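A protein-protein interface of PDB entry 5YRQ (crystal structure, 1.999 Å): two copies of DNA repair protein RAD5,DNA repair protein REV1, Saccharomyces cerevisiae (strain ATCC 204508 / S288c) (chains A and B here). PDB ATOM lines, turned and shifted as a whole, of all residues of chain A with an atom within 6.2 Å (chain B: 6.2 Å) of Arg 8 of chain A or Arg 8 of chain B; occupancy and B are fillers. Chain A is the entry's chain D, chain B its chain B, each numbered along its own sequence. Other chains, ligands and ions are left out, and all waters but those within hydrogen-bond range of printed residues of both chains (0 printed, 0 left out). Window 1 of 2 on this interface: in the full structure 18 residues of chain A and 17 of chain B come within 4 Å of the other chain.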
ATOM      1  N   HIS A   2       7.037  -0.576  -2.273  1.00  0.00           N
ATOM      2  CA  HIS A   2       8.146   0.345  -2.458  1.00  0.00           C
ATOM      3  C   HIS A   2       9.452  -0.423  -2.329  1.00  0.00           C
ATOM      4  O   HIS A   2       9.497  -1.547  -1.816  1.00  0.00           O
ATOM      5  CB  HIS A   2       8.097   1.489  -1.439  1.00  0.00           C
ATOM      6  CG  HIS A   2       8.292   1.037  -0.025  1.00  0.00           C
ATOM      7  ND1 HIS A   2       7.285   0.467   0.726  1.00  0.00           N
ATOM      8  CD2 HIS A   2       9.381   1.074   0.777  1.00  0.00           C
ATOM      9  CE1 HIS A   2       7.749   0.164   1.925  1.00  0.00           C
ATOM     10  NE2 HIS A   2       9.018   0.524   1.983  1.00  0.00           N
ATOM     11  N   MET A   3      10.518   0.209  -2.809  1.00  0.00           N
ATOM     12  CA  MET A   3      11.825  -0.420  -2.900  1.00  0.00           C
ATOM     13  C   MET A   3      12.658  -0.021  -1.689  1.00  0.00           C
ATOM     14  O   MET A   3      12.624   1.133  -1.254  1.00  0.00           O
ATOM     15  CB  MET A   3      12.528   0.003  -4.193  1.00  0.00           C
ATOM     16  CG  MET A   3      13.262  -1.116  -4.919  1.00  0.00           C
ATOM     17  SD  MET A   3      12.204  -2.509  -5.373  1.00  0.00           S
ATOM     18  CE  MET A   3      10.731  -1.648  -5.952  1.00  0.00           C
ATOM     19  N   GLU A   4      13.380  -0.983  -1.122  1.00  0.00           N
ATOM     20  CA  GLU A   4      14.216  -0.705   0.036  1.00  0.00           C
ATOM     21  C   GLU A   4      15.573  -1.368  -0.127  1.00  0.00           C
ATOM     22  O   GLU A   4      15.674  -2.473  -0.664  1.00  0.00           O
ATOM     23  CB  GLU A   4      13.550  -1.173   1.332  1.00  0.00           C
ATOM     24  CG  GLU A   4      12.408  -0.281   1.778  1.00  0.00           C
ATOM     25  CD  GLU A   4      11.903  -0.628   3.165  1.00  0.00           C
ATOM     26  OE1 GLU A   4      10.682  -0.512   3.403  1.00  0.00           O
ATOM     27  OE2 GLU A   4      12.729  -1.022   4.022  1.00  0.00           O
ATOM     28  N   GLN A   5      16.613  -0.678   0.330  1.00  0.00           N
ATOM     29  CA  GLN A   5      17.964  -1.207   0.287  1.00  0.00           C
ATOM     30  C   GLN A   5      18.230  -1.981   1.569  1.00  0.00           C
ATOM     31  O   GLN A   5      17.790  -1.583   2.653  1.00  0.00           O
ATOM     32  CB  GLN A   5      18.988  -0.083   0.118  1.00  0.00           C
ATOM     33  CG  GLN A   5      19.082   0.441  -1.310  1.00  0.00           C
ATOM     34  CD  GLN A   5      20.314   1.294  -1.552  1.00  0.00           C
ATOM     35  OE1 GLN A   5      21.376   1.059  -0.970  1.00  0.00           O
ATOM     36  NE2 GLN A   5      20.175   2.304  -2.406  1.00  0.00           N
ATOM     37  N   GLU A   6      18.920  -3.110   1.435  1.00  0.00           N
ATOM     38  CA  GLU A   6      19.303  -3.905   2.589  1.00  0.00           C
ATOM     39  C   GLU A   6      20.609  -4.622   2.279  1.00  0.00           C
ATOM     40  O   GLU A   6      21.043  -4.698   1.127  1.00  0.00           O
ATOM     41  CB  GLU A   6      18.187  -4.882   2.967  1.00  0.00           C
ATOM     42  CG  GLU A   6      17.635  -5.670   1.792  1.00  0.00           C
ATOM     43  CD  GLU A   6      16.482  -6.580   2.190  1.00  0.00           C
ATOM     44  OE1 GLU A   6      16.743  -7.730   2.597  1.00  0.00           O
ATOM     45  OE2 GLU A   6      15.317  -6.137   2.119  1.00  0.00           O
ATOM     46  N   GLU A   7      21.251  -5.119   3.332  1.00  0.00           N
ATOM     47  CA  GLU A   7      22.443  -5.947   3.222  1.00  0.00           C
ATOM     48  C   GLU A   7      22.076  -7.369   3.613  1.00  0.00           C
ATOM     49  O   GLU A   7      21.455  -7.586   4.659  1.00  0.00           O
ATOM     50  CB  GLU A   7      23.556  -5.410   4.119  1.00  0.00           C
ATOM     51  CG  GLU A   7      24.836  -5.088   3.386  1.00  0.00           C
ATOM     52  CD  GLU A   7      25.755  -4.203   4.206  1.00  0.00           C
ATOM     53  OE1 GLU A   7      26.231  -4.659   5.269  1.00  0.00           O
ATOM     54  OE2 GLU A   7      25.978  -3.043   3.795  1.00  0.00           O
ATOM     55  N   ARG A   8      22.462  -8.334   2.793  1.00  0.00           N
ATOM     56  CA  ARG A   8      22.079  -9.715   3.035  1.00  0.00           C
ATOM     57  C   ARG A   8      23.268 -10.639   2.842  1.00  0.00           C
ATOM     58  O   ARG A   8      24.132 -10.395   1.998  1.00  0.00           O
ATOM     59  CB  ARG A   8      20.930 -10.126   2.116  1.00  0.00           C
ATOM     60  CG  ARG A   8      19.577  -9.681   2.631  1.00  0.00           C
ATOM     61  CD  ARG A   8      18.532 -10.734   2.371  1.00  0.00           C
ATOM     62  NE  ARG A   8      18.123 -10.708   0.975  1.00  0.00           N
ATOM     63  CZ  ARG A   8      17.393 -11.652   0.397  1.00  0.00           C
ATOM     64  NH1 ARG A   8      17.005 -12.707   1.101  1.00  0.00           N
ATOM     65  NH2 ARG A   8      17.055 -11.543  -0.880  1.00  0.00           N
ATOM     66  N   LYS A   9      23.287 -11.717   3.624  1.00  0.00           N
ATOM     67  CA  LYS A   9      24.390 -12.663   3.585  1.00  0.00           C
ATOM     68  C   LYS A   9      24.248 -13.584   2.379  1.00  0.00           C
ATOM     69  O   LYS A   9      23.175 -14.138   2.123  1.00  0.00           O
ATOM     70  CB  LYS A   9      24.441 -13.470   4.885  1.00  0.00           C
ATOM     71  CG  LYS A   9      25.654 -14.361   5.012  1.00  0.00           C
ATOM     72  CD  LYS A   9      25.451 -15.443   6.058  1.00  0.00           C
ATOM     73  CE  LYS A   9      25.204 -14.839   7.435  1.00  0.00           C
ATOM     74  NZ  LYS A   9      24.851 -15.878   8.442  1.00  0.00           N
ATOM     75  N   ARG A  10      25.336 -13.721   1.627  1.00  0.00           N
ATOM     76  CA  ARG A  10      25.423 -14.607   0.473  1.00  0.00           C
ATOM     77  C   ARG A  10      26.567 -15.586   0.698  1.00  0.00           C
ATOM     78  O   ARG A  10      27.631 -15.202   1.197  1.00  0.00           O
ATOM     79  CB  ARG A  10      25.679 -13.828  -0.832  1.00  0.00           C
ATOM     80  CG  ARG A  10      24.498 -13.044  -1.411  1.00  0.00           C
ATOM     81  CD  ARG A  10      23.446 -13.936  -2.042  1.00  0.00           C
ATOM     82  NE  ARG A  10      23.995 -14.905  -2.994  1.00  0.00           N
ATOM     83  CZ  ARG A  10      24.182 -14.664  -4.289  1.00  0.00           C
ATOM     84  NH1 ARG A  10      23.907 -13.464  -4.784  1.00  0.00           N
ATOM     85  NH2 ARG A  10      24.668 -15.613  -5.081  1.00  0.00           N
ATOM     86  N   PRO A  66      18.333 -19.916   3.561  1.00  0.00           N
ATOM     87  CA  PRO A  66      19.361 -19.390   2.664  1.00  0.00           C
ATOM     88  C   PRO A  66      18.845 -18.290   1.743  1.00  0.00           C
ATOM     89  O   PRO A  66      17.642 -18.046   1.613  1.00  0.00           O
ATOM     90  CB  PRO A  66      19.763 -20.626   1.850  1.00  0.00           C
ATOM     91  CG  PRO A  66      18.511 -21.438   1.787  1.00  0.00           C
ATOM     92  CD  PRO A  66      17.749 -21.175   3.062  1.00  0.00           C
ATOM     93  N   HIS A  67      19.797 -17.623   1.101  1.00  0.00           N
ATOM     94  CA  HIS A  67      19.476 -16.600   0.116  1.00  0.00           C
ATOM     95  C   HIS A  67      19.001 -17.268  -1.168  1.00  0.00           C
ATOM     96  O   HIS A  67      19.624 -18.221  -1.650  1.00  0.00           O
ATOM     97  CB  HIS A  67      20.705 -15.730  -0.147  1.00  0.00           C
ATOM     98  CG  HIS A  67      20.397 -14.431  -0.827  1.00  0.00           C
ATOM     99  ND1 HIS A  67      20.013 -14.356  -2.150  1.00  0.00           N
ATOM    100  CD2 HIS A  67      20.441 -13.155  -0.374  1.00  0.00           C
ATOM    101  CE1 HIS A  67      19.824 -13.090  -2.478  1.00  0.00           C
ATOM    102  NE2 HIS A  67      20.079 -12.340  -1.420  1.00  0.00           N
ATOM    103  N   GLU A  68      17.887 -16.771  -1.717  1.00  0.00           N
ATOM    104  CA  GLU A  68      17.315 -17.385  -2.914  1.00  0.00           C
ATOM    105  C   GLU A  68      18.294 -17.416  -4.087  1.00  0.00           C
ATOM    106  O   GLU A  68      18.220 -18.323  -4.922  1.00  0.00           O
ATOM    107  CB  GLU A  68      16.027 -16.661  -3.329  1.00  0.00           C
ATOM    108  CG  GLU A  68      16.184 -15.184  -3.644  1.00  0.00           C
ATOM    109  CD  GLU A  68      16.124 -14.293  -2.409  1.00  0.00           C
ATOM    110  OE1 GLU A  68      16.224 -14.812  -1.273  1.00  0.00           O
ATOM    111  OE2 GLU A  68      15.976 -13.064  -2.586  1.00  0.00           O
ATOM    112  N   HIS B   2      29.663 -13.842   2.723  1.00  0.00           N
ATOM    113  CA  HIS B   2      29.971 -12.429   2.544  1.00  0.00           C
ATOM    114  C   HIS B   2      28.669 -11.647   2.438  1.00  0.00           C
ATOM    115  O   HIS B   2      27.612 -12.199   2.119  1.00  0.00           O
ATOM    116  CB  HIS B   2      30.829 -12.202   1.298  1.00  0.00           C
ATOM    117  CG  HIS B   2      30.151 -12.619   0.034  1.00  0.00           C
ATOM    118  ND1 HIS B   2      30.132 -13.930  -0.391  1.00  0.00           N
ATOM    119  CD2 HIS B   2      29.419 -11.919  -0.868  1.00  0.00           C
ATOM    120  CE1 HIS B   2      29.443 -14.016  -1.514  1.00  0.00           C
ATOM    121  NE2 HIS B   2      29.001 -12.811  -1.825  1.00  0.00           N
ATOM    122  N   MET B   3      28.773 -10.347   2.671  1.00  0.00           N
ATOM    123  CA  MET B   3      27.626  -9.454   2.721  1.00  0.00           C
ATOM    124  C   MET B   3      27.460  -8.767   1.374  1.00  0.00           C
ATOM    125  O   MET B   3      28.439  -8.338   0.758  1.00  0.00           O
ATOM    126  CB  MET B   3      27.816  -8.428   3.843  1.00  0.00           C
ATOM    127  CG  MET B   3      26.553  -7.981   4.569  1.00  0.00           C
ATOM    128  SD  MET B   3      25.440  -9.235   5.259  1.00  0.00           S
ATOM    129  CE  MET B   3      26.559 -10.429   5.946  1.00  0.00           C
ATOM    130  N   GLU B   4      26.217  -8.666   0.916  1.00  0.00           N
ATOM    131  CA  GLU B   4      25.938  -8.037  -0.362  1.00  0.00           C
ATOM    132  C   GLU B   4      24.748  -7.105  -0.211  1.00  0.00           C
ATOM    133  O   GLU B   4      23.773  -7.434   0.469  1.00  0.00           O
ATOM    134  CB  GLU B   4      25.664  -9.096  -1.436  1.00  0.00           C
ATOM    135  CG  GLU B   4      25.290  -8.541  -2.805  1.00  0.00           C
ATOM    136  CD  GLU B   4      25.392  -9.587  -3.896  1.00  0.00           C
ATOM    137  OE1 GLU B   4      26.302 -10.441  -3.808  1.00  0.00           O
ATOM    138  OE2 GLU B   4      24.562  -9.558  -4.830  1.00  0.00           O
ATOM    139  N   GLN B   5      24.829  -5.948  -0.858  1.00  0.00           N
ATOM    140  CA  GLN B   5      23.753  -4.975  -0.814  1.00  0.00           C
ATOM    141  C   GLN B   5      22.790  -5.230  -1.958  1.00  0.00           C
ATOM    142  O   GLN B   5      23.204  -5.536  -3.078  1.00  0.00           O
ATOM    143  CB  GLN B   5      24.299  -3.549  -0.891  1.00  0.00           C
ATOM    144  CG  GLN B   5      24.859  -3.038   0.426  1.00  0.00           C
ATOM    145  CD  GLN B   5      25.082  -1.538   0.427  1.00  0.00           C
ATOM    146  OE1 GLN B   5      24.346  -0.784  -0.214  1.00  0.00           O
ATOM    147  NE2 GLN B   5      26.103  -1.096   1.154  1.00  0.00           N
ATOM    148  N   GLU B   6      21.498  -5.109  -1.676  1.00  0.00           N
ATOM    149  CA  GLU B   6      20.529  -5.260  -2.745  1.00  0.00           C
ATOM    150  C   GLU B   6      19.315  -4.395  -2.462  1.00  0.00           C
ATOM    151  O   GLU B   6      19.116  -3.903  -1.349  1.00  0.00           O
ATOM    152  CB  GLU B   6      20.118  -6.724  -2.944  1.00  0.00           C
ATOM    153  CG  GLU B   6      19.654  -7.457  -1.700  1.00  0.00           C
ATOM    154  CD  GLU B   6      19.339  -8.917  -1.991  1.00  0.00           C
ATOM    155  OE1 GLU B   6      18.204  -9.216  -2.418  1.00  0.00           O
ATOM    156  OE2 GLU B   6      20.226  -9.768  -1.782  1.00  0.00           O
ATOM    157  N   GLU B   7      18.506  -4.223  -3.500  1.00  0.00           N
ATOM    158  CA  GLU B   7      17.229  -3.535  -3.419  1.00  0.00           C
ATOM    159  C   GLU B   7      16.125  -4.571  -3.454  1.00  0.00           C
ATOM    160  O   GLU B   7      16.149  -5.478  -4.290  1.00  0.00           O
ATOM    161  CB  GLU B   7      17.044  -2.573  -4.587  1.00  0.00           C
ATOM    162  CG  GLU B   7      16.699  -1.167  -4.187  1.00  0.00           C
ATOM    163  CD  GLU B   7      16.866  -0.205  -5.334  1.00  0.00           C
ATOM    164  OE1 GLU B   7      16.141  -0.375  -6.338  1.00  0.00           O
ATOM    165  OE2 GLU B   7      17.697   0.720  -5.230  1.00  0.00           O
ATOM    166  N   ARG B   8      15.182  -4.459  -2.532  1.00  0.00           N
ATOM    167  CA  ARG B   8      14.104  -5.425  -2.470  1.00  0.00           C
ATOM    168  C   ARG B   8      12.787  -4.703  -2.260  1.00  0.00           C
ATOM    169  O   ARG B   8      12.721  -3.669  -1.590  1.00  0.00           O
ATOM    170  CB  ARG B   8      14.359  -6.460  -1.380  1.00  0.00           C
ATOM    171  CG  ARG B   8      15.286  -7.552  -1.850  1.00  0.00           C
ATOM    172  CD  ARG B   8      14.826  -8.869  -1.305  1.00  0.00           C
ATOM    173  NE  ARG B   8      15.193  -8.966   0.100  1.00  0.00           N
ATOM    174  CZ  ARG B   8      14.731  -9.890   0.933  1.00  0.00           C
ATOM    175  NH1 ARG B   8      15.128  -9.897   2.198  1.00  0.00           N
ATOM    176  NH2 ARG B   8      13.864 -10.796   0.503  1.00  0.00           N
ATOM    177  N   LYS B   9      11.738  -5.270  -2.844  1.00  0.00           N
ATOM    178  CA  LYS B   9      10.412  -4.681  -2.776  1.00  0.00           C
ATOM    179  C   LYS B   9       9.800  -4.986  -1.416  1.00  0.00           C
ATOM    180  O   LYS B   9       9.809  -6.135  -0.964  1.00  0.00           O
ATOM    181  CB  LYS B   9       9.530  -5.239  -3.894  1.00  0.00           C
ATOM    182  CG  LYS B   9       8.171  -4.585  -4.011  1.00  0.00           C
ATOM    183  CD  LYS B   9       7.173  -5.483  -4.738  1.00  0.00           C
ATOM    184  CE  LYS B   9       7.597  -5.822  -6.158  1.00  0.00           C
ATOM    185  NZ  LYS B   9       6.675  -6.827  -6.775  1.00  0.00           N
ATOM    186  N   ARG B  10       9.272  -3.957  -0.767  1.00  0.00           N
ATOM    187  CA  ARG B  10       8.579  -4.103   0.504  1.00  0.00           C
ATOM    188  C   ARG B  10       7.150  -3.639   0.289  1.00  0.00           C
ATOM    189  O   ARG B  10       6.918  -2.570  -0.286  1.00  0.00           O
ATOM    190  CB  ARG B  10       9.239  -3.280   1.617  1.00  0.00           C
ATOM    191  CG  ARG B  10      10.532  -3.855   2.200  1.00  0.00           C
ATOM    192  CD  ARG B  10      10.268  -5.059   3.086  1.00  0.00           C
ATOM    193  NE  ARG B  10       9.229  -4.808   4.080  1.00  0.00           N
ATOM    194  CZ  ARG B  10       9.450  -4.297   5.289  1.00  0.00           C
ATOM    195  NH1 ARG B  10      10.676  -3.949   5.660  1.00  0.00           N
ATOM    196  NH2 ARG B  10       8.439  -4.124   6.125  1.00  0.00           N
ATOM    197  N   PRO B  66       6.766 -13.361  -0.920  1.00  0.00           N
ATOM    198  CA  PRO B  66       6.806 -12.064  -0.249  1.00  0.00           C
ATOM    199  C   PRO B  66       8.083 -11.896   0.561  1.00  0.00           C
ATOM    200  O   PRO B  66       8.843 -12.837   0.775  1.00  0.00           O
ATOM    201  CB  PRO B  66       5.581 -12.127   0.666  1.00  0.00           C
ATOM    202  CG  PRO B  66       5.505 -13.556   1.044  1.00  0.00           C
ATOM    203  CD  PRO B  66       6.024 -14.356  -0.133  1.00  0.00           C
ATOM    204  N   HIS B  67       8.297 -10.664   1.007  1.00  0.00           N
ATOM    205  CA  HIS B  67       9.457 -10.316   1.812  1.00  0.00           C
ATOM    206  C   HIS B  67       9.242 -10.797   3.242  1.00  0.00           C
ATOM    207  O   HIS B  67       8.184 -10.553   3.824  1.00  0.00           O
ATOM    208  CB  HIS B  67       9.655  -8.801   1.770  1.00  0.00           C
ATOM    209  CG  HIS B  67      10.989  -8.341   2.267  1.00  0.00           C
ATOM    210  ND1 HIS B  67      11.359  -8.421   3.592  1.00  0.00           N
ATOM    211  CD2 HIS B  67      12.030  -7.768   1.616  1.00  0.00           C
ATOM    212  CE1 HIS B  67      12.577  -7.926   3.734  1.00  0.00           C
ATOM    213  NE2 HIS B  67      13.005  -7.520   2.551  1.00  0.00           N
ATOM    214  N   GLU B  68      10.245 -11.471   3.819  1.00  0.00           N
ATOM    215  CA  GLU B  68      10.047 -12.043   5.152  1.00  0.00           C
ATOM    216  C   GLU B  68       9.695 -10.982   6.200  1.00  0.00           C
ATOM    217  O   GLU B  68       8.998 -11.292   7.172  1.00  0.00           O
ATOM    218  CB  GLU B  68      11.285 -12.834   5.595  1.00  0.00           C
ATOM    219  CG  GLU B  68      12.563 -12.022   5.725  1.00  0.00           C
ATOM    220  CD  GLU B  68      13.298 -11.857   4.404  1.00  0.00           C
ATOM    221  OE1 GLU B  68      12.727 -12.220   3.353  1.00  0.00           O
ATOM    222  OE2 GLU B  68      14.452 -11.367   4.418  1.00  0.00           O
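The backbone NH (N) of Lys 9 of chain A lies within hydrogen-bond range of the side-chain sulfur (SD) of Met 3 of chain B (3.7 Å).
The guanidinium group (NH2) of Arg 8 of chain A lies within salt-bridge range of the side-chain carboxylate (OE1) of Glu 6 of chain B (3.0 Å).
OE2 of Glu 4 of chain A is in salt-bridge range of NH1 of Arg 10 of chain B, at 3.9 Å.
A ring nitrogen (NE2) of His 67 of chain A sits at hydrogen-bond distance from the side-chain carboxylate of Glu 6 of chain B (2.6 Å).
O of His 2 of chain A is in hydrogen-bond range of N of Arg 10 of chain B.
The guanidinium group of Arg 8 of chain B is in salt-bridge range of the side-chain carboxylate of Glu 6 of chain A (2.7 Å).
NE2 of His 67 of chain B sits at hydrogen-bond distance from OE2 of Glu 6 of chain A.
The backbone NH (N) of Arg 10 of chain A is in hydrogen-bond range of the backbone carbonyl oxygen (O) of His 2 of chain B, at 2.8 Å.
N of Arg 8 of chain A sits at hydrogen-bond distance from O of Glu 4 of chain B (2.8 Å).
The backbone NH of Arg 8 of chain B is in hydrogen-bond range of the backbone carbonyl oxygen of Glu 4 of chain A, at 2.8 Å.
N of Lys 9 of chain B is in hydrogen-bond range of SD of Met 3 of chain A (3.8 Å).
The side-chain carboxylate of Glu 4 of chain B lies within salt-bridge range of the guanidinium group of Arg 10 of chain A (3.96 Å).
NE2 of Gln 5 of chain B is in hydrogen-bond range of OE2 of Glu 7 of chain A, at 3.3 Å.
The side-chain sulfur of Met 3 of chain B sits close to the backbone carbonyl oxygen of Arg 8 of chain A (3.7 Å).
NE of Arg 8 of chain B sits close to NH2 of Arg 8 of chain A, at 3.3 Å.
The backbone NH of Glu 6 of chain B is in hydrogen-bond range of the backbone carbonyl oxygen of Glu 6 of chain A.
His 2 of chain A touches Arg 8 of chain B (O to O, 3.9 Å).
Glu 7 of chain B touches Met 3 of chain A (OE1 to CG, 3.3 Å).
Met 3 of chain A touches Arg 8 of chain B.
O of Glu 6 of chain B touches O of Glu 4 of chain A, 3.8 Å away.
Gln 5 of chain A touches Glu 6 of chain B (CA to O, 3.4 Å).
CA of Gln 5 of chain B touches O of Glu 6 of chain A, 3.3 Å away.
Met 3 of chain B touches Glu 7 of chain A.
Glu 7 of chain A touches Glu 4 of chain B (CA to O, 3.4 Å).
His 2 of chain B touches Arg 8 of chain A.
His 2 of chain B touches Lys 9 of chain A.
OE1 of Glu 6 of chain B lies within salt-bridge range of NE of Arg 8 of chain B, 3.9 Å away.
The guanidinium group of Arg 8 of chain A lies within salt-bridge range of the side-chain carboxylate of Glu 68 of chain A (2.5 Å).
NE2 of His 2 of chain A lies within hydrogen-bond range of OE1 of Glu 4 of chain A, at 2.4 Å.
NE2 of His 67 of chain A lies within hydrogen-bond range of NH2 of Arg 8 of chain A, 3.2 Å away.
OE1 of Glu 6 of chain A lies within salt-bridge range of NE of Arg 8 of chain A (3.7 Å).
NH1 of Arg 8 of chain B lies within hydrogen-bond range of NE2 of His 67 of chain B (3.2 Å).
Of the 12 printed residues of chain B, 10 touch a printed residue of chain A.
Hydrophobic or aromatic side chains of chain B that line the printed part of chain A: His 2, Met 3 and His 67.
Among the printed residues, Asp or Glu carboxylates within 4 Å of a Lys or Arg side-chain nitrogen of the other chain: Glu 4 of chain A with Arg 10 of chain B, Glu 6 of chain A with Arg 8 of chain B, Arg 8 of chain A with Glu 6 of chain B and Arg 10 of chain A with Glu 4 of chain B.
Arg 8 of chain A touches just these residues of chain B: His 2, Met 3, Glu 4, Glu 6 and Arg 8.
Pro 66 of chain A touches none of the printed residues of chain B.
Printed residues of chain A within 4 Å of Glu 4 of chain B: Glu 6 (3.9 Å), Glu 7 (3.4 Å), Arg 8 (2.8 Å) and Arg 10 (3.96 Å).
Arg 8 of chain B touches just these residues of chain A: His 2 (3.9 Å), Met 3 (3.6 Å), Glu 4 (2.8 Å), Glu 6 (2.7 Å) and Arg 8 (3.2 Å).
Pro 66 of chain B touches none of the printed residues of chain A.
Of the printed residues of chain A, His 67 of chain B touches Glu 6 (2.7 Å).
The nearest residue of chain B that does not touch Arg 8 of chain A is Glu 68 of chain B (4.4 Å).
The nearest printed residue of chain A that does not touch His 67 of chain B is Arg 8 of chain A (6.2 Å).
Glu 4 of chain A touches Arg 8 of chain B, and with the chains exchanged Arg 8 of chain A touches Glu 4 of chain B.
Glu 6 of chain A touches Arg 8 of chain B, and with the chains exchanged Arg 8 of chain A touches Glu 6 of chain B.
Glu 7 of chain A touches Gln 5 of chain B, but with the chains exchanged Gln 5 of chain A does not touch Glu 7 of chain B (4.1 Å).
Arg 8 of chain A touches its own counterpart, Arg 8 of chain B.
Of the 30 pairs that touch across the chains among the printed residues, 29 have their exchanged pair printed and touching as well.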
